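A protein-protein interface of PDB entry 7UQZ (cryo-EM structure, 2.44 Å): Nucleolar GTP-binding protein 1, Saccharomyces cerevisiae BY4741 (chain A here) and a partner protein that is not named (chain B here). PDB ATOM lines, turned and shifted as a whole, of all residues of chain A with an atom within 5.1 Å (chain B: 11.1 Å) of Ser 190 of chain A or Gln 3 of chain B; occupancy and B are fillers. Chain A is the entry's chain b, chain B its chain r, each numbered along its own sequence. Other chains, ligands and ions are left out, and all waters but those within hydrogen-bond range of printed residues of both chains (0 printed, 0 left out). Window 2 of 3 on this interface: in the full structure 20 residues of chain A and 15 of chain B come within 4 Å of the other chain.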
ATOM      1  N   ARG A 159      -1.146  -9.465  16.334  1.00  0.00           N
ATOM      2  CA  ARG A 159      -1.614  -8.298  17.065  1.00  0.00           C
ATOM      3  C   ARG A 159      -1.526  -8.465  18.578  1.00  0.00           C
ATOM      4  O   ARG A 159      -1.988  -7.586  19.311  1.00  0.00           O
ATOM      5  CB  ARG A 159      -3.052  -7.973  16.661  1.00  0.00           C
ATOM      6  CG  ARG A 159      -3.275  -7.951  15.161  1.00  0.00           C
ATOM      7  CD  ARG A 159      -4.628  -7.376  14.814  1.00  0.00           C
ATOM      8  NE  ARG A 159      -5.723  -8.081  15.467  1.00  0.00           N
ATOM      9  CZ  ARG A 159      -6.439  -9.046  14.907  1.00  0.00           C
ATOM     10  NH1 ARG A 159      -6.198  -9.460  13.673  1.00  0.00           N
ATOM     11  NH2 ARG A 159      -7.425  -9.608  15.600  1.00  0.00           N
ATOM     12  N   PRO A 161      -0.079  -8.183  22.231  1.00  0.00           N
ATOM     13  CA  PRO A 161       0.894  -7.276  22.846  1.00  0.00           C
ATOM     14  C   PRO A 161       2.138  -8.019  23.302  1.00  0.00           C
ATOM     15  O   PRO A 161       2.085  -9.188  23.694  1.00  0.00           O
ATOM     16  CB  PRO A 161       0.130  -6.689  24.036  1.00  0.00           C
ATOM     17  CG  PRO A 161      -0.899  -7.709  24.359  1.00  0.00           C
ATOM     18  CD  PRO A 161      -1.292  -8.333  23.052  1.00  0.00           C
ATOM     19  N   LEU A 184      -5.241   1.737  34.536  1.00  0.00           N
ATOM     20  CA  LEU A 184      -4.243   1.603  33.478  1.00  0.00           C
ATOM     21  C   LEU A 184      -4.180   2.862  32.620  1.00  0.00           C
ATOM     22  O   LEU A 184      -3.092   3.303  32.234  1.00  0.00           O
ATOM     23  CB  LEU A 184      -4.538   0.382  32.609  1.00  0.00           C
ATOM     24  CG  LEU A 184      -3.463   0.118  31.548  1.00  0.00           C
ATOM     25  CD1 LEU A 184      -2.186  -0.394  32.199  1.00  0.00           C
ATOM     26  CD2 LEU A 184      -3.945  -0.830  30.464  1.00  0.00           C
ATOM     27  N   ARG A 185      -5.338   3.451  32.311  1.00  0.00           N
ATOM     28  CA  ARG A 185      -5.361   4.721  31.590  1.00  0.00           C
ATOM     29  C   ARG A 185      -4.700   5.831  32.397  1.00  0.00           C
ATOM     30  O   ARG A 185      -4.012   6.691  31.835  1.00  0.00           O
ATOM     31  CB  ARG A 185      -6.795   5.114  31.251  1.00  0.00           C
ATOM     32  CG  ARG A 185      -7.329   4.566  29.949  1.00  0.00           C
ATOM     33  CD  ARG A 185      -8.612   5.291  29.592  1.00  0.00           C
ATOM     34  NE  ARG A 185      -9.332   4.658  28.497  1.00  0.00           N
ATOM     35  CZ  ARG A 185     -10.521   5.053  28.063  1.00  0.00           C
ATOM     36  NH1 ARG A 185     -11.144   6.087  28.605  1.00  0.00           N
ATOM     37  NH2 ARG A 185     -11.099   4.395  27.063  1.00  0.00           N
ATOM     38  N   THR A 188      -0.728   4.919  32.489  1.00  0.00           N
ATOM     39  CA  THR A 188      -0.046   4.695  31.220  1.00  0.00           C
ATOM     40  C   THR A 188      -0.715   5.498  30.113  1.00  0.00           C
ATOM     41  O   THR A 188      -1.584   6.333  30.382  1.00  0.00           O
ATOM     42  CB  THR A 188      -0.042   3.209  30.845  1.00  0.00           C
ATOM     43  OG1 THR A 188      -1.392   2.742  30.728  1.00  0.00           O
ATOM     44  CG2 THR A 188       0.691   2.375  31.888  1.00  0.00           C
ATOM     45  N   LYS A 189      -0.316   5.255  28.864  1.00  0.00           N
ATOM     46  CA  LYS A 189      -0.977   5.846  27.706  1.00  0.00           C
ATOM     47  C   LYS A 189      -1.620   4.786  26.820  1.00  0.00           C
ATOM     48  O   LYS A 189      -1.819   5.019  25.623  1.00  0.00           O
ATOM     49  CB  LYS A 189       0.000   6.701  26.899  1.00  0.00           C
ATOM     50  CG  LYS A 189       1.321   6.031  26.591  1.00  0.00           C
ATOM     51  CD  LYS A 189       2.197   6.935  25.740  1.00  0.00           C
ATOM     52  CE  LYS A 189       2.356   8.309  26.372  1.00  0.00           C
ATOM     53  NZ  LYS A 189       3.141   9.230  25.506  1.00  0.00           N
ATOM     54  N   SER A 190      -1.939   3.624  27.381  1.00  0.00           N
ATOM     55  CA  SER A 190      -2.673   2.604  26.648  1.00  0.00           C
ATOM     56  C   SER A 190      -4.094   3.074  26.362  1.00  0.00           C
ATOM     57  O   SER A 190      -4.675   3.867  27.107  1.00  0.00           O
ATOM     58  CB  SER A 190      -2.699   1.295  27.438  1.00  0.00           C
ATOM     59  OG  SER A 190      -3.482   0.315  26.779  1.00  0.00           O
ATOM     60  N   ASP A 191      -4.655   2.578  25.261  1.00  0.00           N
ATOM     61  CA  ASP A 191      -5.981   2.984  24.799  1.00  0.00           C
ATOM     62  C   ASP A 191      -7.045   1.942  25.119  1.00  0.00           C
ATOM     63  O   ASP A 191      -7.945   1.692  24.313  1.00  0.00           O
ATOM     64  CB  ASP A 191      -5.950   3.280  23.302  1.00  0.00           C
ATOM     65  CG  ASP A 191      -5.527   2.081  22.480  1.00  0.00           C
ATOM     66  OD1 ASP A 191      -4.745   1.254  22.995  1.00  0.00           O
ATOM     67  OD2 ASP A 191      -5.980   1.963  21.322  1.00  0.00           O
ATOM     68  N   VAL A 192      -6.959   1.313  26.292  1.00  0.00           N
ATOM     69  CA  VAL A 192      -7.950   0.318  26.684  1.00  0.00           C
ATOM     70  C   VAL A 192      -9.283   1.005  26.963  1.00  0.00           C
ATOM     71  O   VAL A 192      -9.332   2.117  27.507  1.00  0.00           O
ATOM     72  CB  VAL A 192      -7.442  -0.486  27.897  1.00  0.00           C
ATOM     73  CG1 VAL A 192      -7.207   0.415  29.105  1.00  0.00           C
ATOM     74  CG2 VAL A 192      -8.391  -1.628  28.236  1.00  0.00           C
ATOM     75  N   LEU A 204      -5.522  -9.418  27.568  1.00  0.00           N
ATOM     76  CA  LEU A 204      -4.505  -8.659  28.284  1.00  0.00           C
ATOM     77  C   LEU A 204      -4.158  -7.379  27.532  1.00  0.00           C
ATOM     78  O   LEU A 204      -4.043  -7.370  26.304  1.00  0.00           O
ATOM     79  CB  LEU A 204      -3.249  -9.510  28.474  1.00  0.00           C
ATOM     80  CG  LEU A 204      -3.430 -10.890  29.108  1.00  0.00           C
ATOM     81  CD1 LEU A 204      -2.133 -11.673  29.051  1.00  0.00           C
ATOM     82  CD2 LEU A 204      -3.914 -10.758  30.538  1.00  0.00           C
ATOM     83  N   TYR A 205      -4.001  -6.289  28.279  1.00  0.00           N
ATOM     84  CA  TYR A 205      -3.572  -5.010  27.728  1.00  0.00           C
ATOM     85  C   TYR A 205      -2.326  -4.545  28.463  1.00  0.00           C
ATOM     86  O   TYR A 205      -2.203  -4.733  29.675  1.00  0.00           O
ATOM     87  CB  TYR A 205      -4.673  -3.950  27.833  1.00  0.00           C
ATOM     88  CG  TYR A 205      -5.684  -3.993  26.709  1.00  0.00           C
ATOM     89  CD1 TYR A 205      -6.705  -4.930  26.705  1.00  0.00           C
ATOM     90  CD2 TYR A 205      -5.619  -3.092  25.654  1.00  0.00           C
ATOM     91  CE1 TYR A 205      -7.633  -4.973  25.686  1.00  0.00           C
ATOM     92  CE2 TYR A 205      -6.541  -3.126  24.629  1.00  0.00           C
ATOM     93  CZ  TYR A 205      -7.546  -4.068  24.650  1.00  0.00           C
ATOM     94  OH  TYR A 205      -8.469  -4.110  23.632  1.00  0.00           O
ATOM     95  N   VAL A 206      -1.400  -3.939  27.727  1.00  0.00           N
ATOM     96  CA  VAL A 206      -0.093  -3.574  28.257  1.00  0.00           C
ATOM     97  C   VAL A 206       0.079  -2.066  28.162  1.00  0.00           C
ATOM     98  O   VAL A 206      -0.286  -1.452  27.154  1.00  0.00           O
ATOM     99  CB  VAL A 206       1.042  -4.302  27.506  1.00  0.00           C
ATOM    100  CG1 VAL A 206       2.393  -3.999  28.135  1.00  0.00           C
ATOM    101  CG2 VAL A 206       0.792  -5.792  27.496  1.00  0.00           C
ATOM    102  N   GLY A 207       0.606  -1.469  29.235  1.00  0.00           N
ATOM    103  CA  GLY A 207       1.073  -0.104  29.201  1.00  0.00           C
ATOM    104  C   GLY A 207       2.455  -0.025  29.826  1.00  0.00           C
ATOM    105  O   GLY A 207       2.925  -0.976  30.447  1.00  0.00           O
ATOM    106  N   PRO B   2       0.218  -0.917  18.614  1.00  0.00           N
ATOM    107  CA  PRO B   2      -1.189  -1.217  18.863  1.00  0.00           C
ATOM    108  C   PRO B   2      -1.371  -2.680  19.248  1.00  0.00           C
ATOM    109  O   PRO B   2      -0.559  -3.520  18.863  1.00  0.00           O
ATOM    110  CB  PRO B   2      -1.843  -0.893  17.529  1.00  0.00           C
ATOM    111  CG  PRO B   2      -0.811  -1.240  16.545  1.00  0.00           C
ATOM    112  CD  PRO B   2       0.520  -0.921  17.176  1.00  0.00           C
ATOM    113  N   GLN B   3      -2.414  -2.978  20.014  1.00  0.00           N
ATOM    114  CA  GLN B   3      -2.635  -4.316  20.539  1.00  0.00           C
ATOM    115  C   GLN B   3      -4.078  -4.736  20.298  1.00  0.00           C
ATOM    116  O   GLN B   3      -4.989  -3.903  20.289  1.00  0.00           O
ATOM    117  CB  GLN B   3      -2.296  -4.381  22.040  1.00  0.00           C
ATOM    118  CG  GLN B   3      -2.760  -3.168  22.840  1.00  0.00           C
ATOM    119  CD  GLN B   3      -2.157  -3.109  24.232  1.00  0.00           C
ATOM    120  OE1 GLN B   3      -1.717  -4.119  24.775  1.00  0.00           O
ATOM    121  NE2 GLN B   3      -2.132  -1.917  24.814  1.00  0.00           N
ATOM    122  N   ASN B   4      -4.265  -6.034  20.082  1.00  0.00           N
ATOM    123  CA  ASN B   4      -5.580  -6.696  19.949  1.00  0.00           C
ATOM    124  C   ASN B   4      -6.283  -6.139  18.704  1.00  0.00           C
ATOM    125  O   ASN B   4      -5.641  -5.975  17.656  1.00  0.00           O
ATOM    126  CB  ASN B   4      -6.343  -6.558  21.250  1.00  0.00           C
ATOM    127  CG  ASN B   4      -5.548  -7.061  22.441  1.00  0.00           C
ATOM    128  OD1 ASN B   4      -4.887  -8.094  22.366  1.00  0.00           O
ATOM    129  ND2 ASN B   4      -5.595  -6.323  23.541  1.00  0.00           N
ATOM    130  N   ASP B   5      -7.586  -5.858  18.766  1.00  0.00           N
ATOM    131  CA  ASP B   5      -8.342  -5.426  17.587  1.00  0.00           C
ATOM    132  C   ASP B   5      -8.345  -3.898  17.493  1.00  0.00           C
ATOM    133  O   ASP B   5      -9.366  -3.220  17.642  1.00  0.00           O
ATOM    134  CB  ASP B   5      -9.753  -5.999  17.626  1.00  0.00           C
ATOM    135  CG  ASP B   5     -10.473  -5.693  18.922  1.00  0.00           C
ATOM    136  OD1 ASP B   5      -9.802  -5.584  19.970  1.00  0.00           O
ATOM    137  OD2 ASP B   5     -11.713  -5.555  18.893  1.00  0.00           O
ATOM    138  N   TYR B   6      -7.156  -3.359  17.209  1.00  0.00           N
ATOM    139  CA  TYR B   6      -6.973  -1.911  17.228  1.00  0.00           C
ATOM    140  C   TYR B   6      -7.671  -1.221  16.061  1.00  0.00           C
ATOM    141  O   TYR B   6      -8.135  -0.090  16.213  1.00  0.00           O
ATOM    142  CB  TYR B   6      -5.483  -1.564  17.252  1.00  0.00           C
ATOM    143  CG  TYR B   6      -4.625  -2.301  16.248  1.00  0.00           C
ATOM    144  CD1 TYR B   6      -4.003  -3.498  16.583  1.00  0.00           C
ATOM    145  CD2 TYR B   6      -4.398  -1.777  14.980  1.00  0.00           C
ATOM    146  CE1 TYR B   6      -3.205  -4.167  15.674  1.00  0.00           C
ATOM    147  CE2 TYR B   6      -3.606  -2.441  14.065  1.00  0.00           C
ATOM    148  CZ  TYR B   6      -3.009  -3.633  14.419  1.00  0.00           C
ATOM    149  OH  TYR B   6      -2.218  -4.296  13.513  1.00  0.00           O
ATOM    150  N   ILE B   7      -7.777  -1.876  14.904  1.00  0.00           N
ATOM    151  CA  ILE B   7      -8.470  -1.269  13.770  1.00  0.00           C
ATOM    152  C   ILE B   7      -9.969  -1.191  14.038  1.00  0.00           C
ATOM    153  O   ILE B   7     -10.614  -0.178  13.740  1.00  0.00           O
ATOM    154  CB  ILE B   7      -8.157  -2.043  12.473  1.00  0.00           C
ATOM    155  CG1 ILE B   7      -6.708  -1.805  12.045  1.00  0.00           C
ATOM    156  CG2 ILE B   7      -9.116  -1.659  11.355  1.00  0.00           C
ATOM    157  CD1 ILE B   7      -6.386  -0.361  11.745  1.00  0.00           C
ATOM    158  N   GLU B   8     -10.544  -2.250  14.611  1.00  0.00           N
ATOM    159  CA  GLU B   8     -11.954  -2.207  14.985  1.00  0.00           C
ATOM    160  C   GLU B   8     -12.203  -1.172  16.074  1.00  0.00           C
ATOM    161  O   GLU B   8     -13.215  -0.462  16.044  1.00  0.00           O
ATOM    162  CB  GLU B   8     -12.430  -3.589  15.428  1.00  0.00           C
ATOM    163  CG  GLU B   8     -12.912  -4.459  14.281  1.00  0.00           C
ATOM    164  CD  GLU B   8     -13.282  -5.861  14.721  1.00  0.00           C
ATOM    165  OE1 GLU B   8     -12.937  -6.242  15.858  1.00  0.00           O
ATOM    166  OE2 GLU B   8     -13.917  -6.584  13.927  1.00  0.00           O
ATOM    167  N   ARG B   9     -11.284  -1.059  17.038  1.00  0.00           N
ATOM    168  CA  ARG B   9     -11.416  -0.015  18.051  1.00  0.00           C
ATOM    169  C   ARG B   9     -11.322   1.375  17.432  1.00  0.00           C
ATOM    170  O   ARG B   9     -12.030   2.296  17.850  1.00  0.00           O
ATOM    171  CB  ARG B   9     -10.356  -0.188  19.138  1.00  0.00           C
ATOM    172  CG  ARG B   9     -10.577  -1.395  20.033  1.00  0.00           C
ATOM    173  CD  ARG B   9      -9.749  -1.303  21.303  1.00  0.00           C
ATOM    174  NE  ARG B   9      -8.330  -1.115  21.027  1.00  0.00           N
ATOM    175  CZ  ARG B   9      -7.453  -2.101  20.905  1.00  0.00           C
ATOM    176  NH1 ARG B   9      -7.819  -3.367  21.014  1.00  0.00           N
ATOM    177  NH2 ARG B   9      -6.178  -1.810  20.669  1.00  0.00           N
ATOM    178  N   HIS B  10     -10.449   1.547  16.438  1.00  0.00           N
ATOM    179  CA  HIS B  10     -10.317   2.836  15.767  1.00  0.00           C
ATOM    180  C   HIS B  10     -11.577   3.184  14.988  1.00  0.00           C
ATOM    181  O   HIS B  10     -11.987   4.347  14.951  1.00  0.00           O
ATOM    182  CB  HIS B  10      -9.102   2.822  14.841  1.00  0.00           C
ATOM    183  CG  HIS B  10      -8.829   4.139  14.185  1.00  0.00           C
ATOM    184  ND1 HIS B  10      -8.056   5.117  14.772  1.00  0.00           N
ATOM    185  CD2 HIS B  10      -9.233   4.643  12.995  1.00  0.00           C
ATOM    186  CE1 HIS B  10      -7.991   6.164  13.971  1.00  0.00           C
ATOM    187  NE2 HIS B  10      -8.698   5.904  12.886  1.00  0.00           N
ATOM    188  N   GLN B  13     -14.155   4.241  17.605  1.00  0.00           N
ATOM    189  CA  GLN B  13     -13.883   5.495  18.300  1.00  0.00           C
ATOM    190  C   GLN B  13     -13.794   6.704  17.376  1.00  0.00           C
ATOM    191  O   GLN B  13     -14.017   7.832  17.829  1.00  0.00           O
ATOM    192  CB  GLN B  13     -12.580   5.375  19.095  1.00  0.00           C
ATOM    193  CG  GLN B  13     -12.667   4.447  20.290  1.00  0.00           C
ATOM    194  CD  GLN B  13     -13.298   5.113  21.494  1.00  0.00           C
ATOM    195  OE1 GLN B  13     -12.929   6.226  21.862  1.00  0.00           O
ATOM    196  NE2 GLN B  13     -14.254   4.434  22.114  1.00  0.00           N
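The backbone NH (N) of Asn 4 of chain B lies within hydrogen-bond range of the backbone carbonyl oxygen (O) of Arg 159 of chain A (2.9 Å). The side-chain hydroxyl (OH) of Tyr 205 of chain A sits at hydrogen-bond distance from the guanidinium group (NH1) of Arg 9 of chain B, 2.8 Å away. The side-chain amide nitrogen (ND2) of Asn 4 of chain B lies within hydrogen-bond range of the backbone carbonyl oxygen (O) of Leu 204 of chain A (3.3 Å). NE2 of Gln 3 of chain B sits at hydrogen-bond distance from OG of Ser 190 of chain A, at 3.3 Å. N of Val 206 of chain A lies within hydrogen-bond range of OE1 of Gln 3 of chain B (3.0 Å). The guanidinium group of Arg 9 of chain B is in salt-bridge range of the side-chain carboxylate of Asp 191 of chain A, at 3.8 Å.
Of the 13 printed residues of chain A, 7 touch a printed residue of chain B. Along chain A the printed residues that touch a printed residue of chain B span positions 159 to 206. Among the printed residues, 12 pairs touch across the chains. Among the printed residues, Asp or Glu carboxylates within 4 Å of a Lys or Arg side-chain nitrogen of the other chain: Asp 191 of chain A with Arg 9 of chain B.
Arg 159 of chain A touches Gln 3 of chain B. CD of Arg 159 of chain A touches CE1 of Tyr 6 of chain B, 3.6 Å away. CB of Pro 161 of chain A touches OE1 of Gln 3 of chain B, 3.2 Å away. Pro 161 of chain A touches Asn 4 of chain B (CD to OD1, 3.7 Å). CA of Tyr 205 of chain A touches OE1 of Gln 3 of chain B (3.6 Å). Asn 4 of chain B touches Tyr 205 of chain A (ND2 to CZ, 3.2 Å).
The guanidinium group (NH2) of Arg 9 of chain B lies within hydrogen-bond range of the backbone carbonyl oxygen (O) of Gln 3 of chain B, at 2.4 Å. The guanidinium group of Arg 9 of chain B lies within salt-bridge range of the side-chain carboxylate of Asp 5 of chain B, 3.2 Å away.
Printed residues of chain B within 4 Å of Ser 190 of chain A: Gln 3 (3.3 Å). Gln 3 of chain B touches five residues of chain A. Of the printed residues of chain B, Pro 161 of chain A touches Gln 3 (3.2 Å) and Asn 4 (3.7 Å). No residue of chain B comes within 4 Å of Thr 188 of chain A. Asp 191 of chain A touches one residue of chain B. Of chain B, only Gln 3, Asn 4 and Arg 9 come within 4 Å of Tyr 205 of chain A. Val 206 of chain A touches just one residue of chain B: Gln 3. No residue of chain B comes within 4 Å of Gly 207 of chain A. Printed residues of chain A within 4 Å of Arg 9 of chain B: Asp 191 (3.8 Å) and Tyr 205 (2.8 Å). Of the printed residues of chain A, Asn 4 of chain B touches Arg 159, Pro 161, Leu 204 and Tyr 205. Lys 189 of chain A touches none of the printed residues of chain B. The nearest printed residue of chain A that does not touch Arg 9 of chain B is Val 192 of chain A (5.8 Å).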
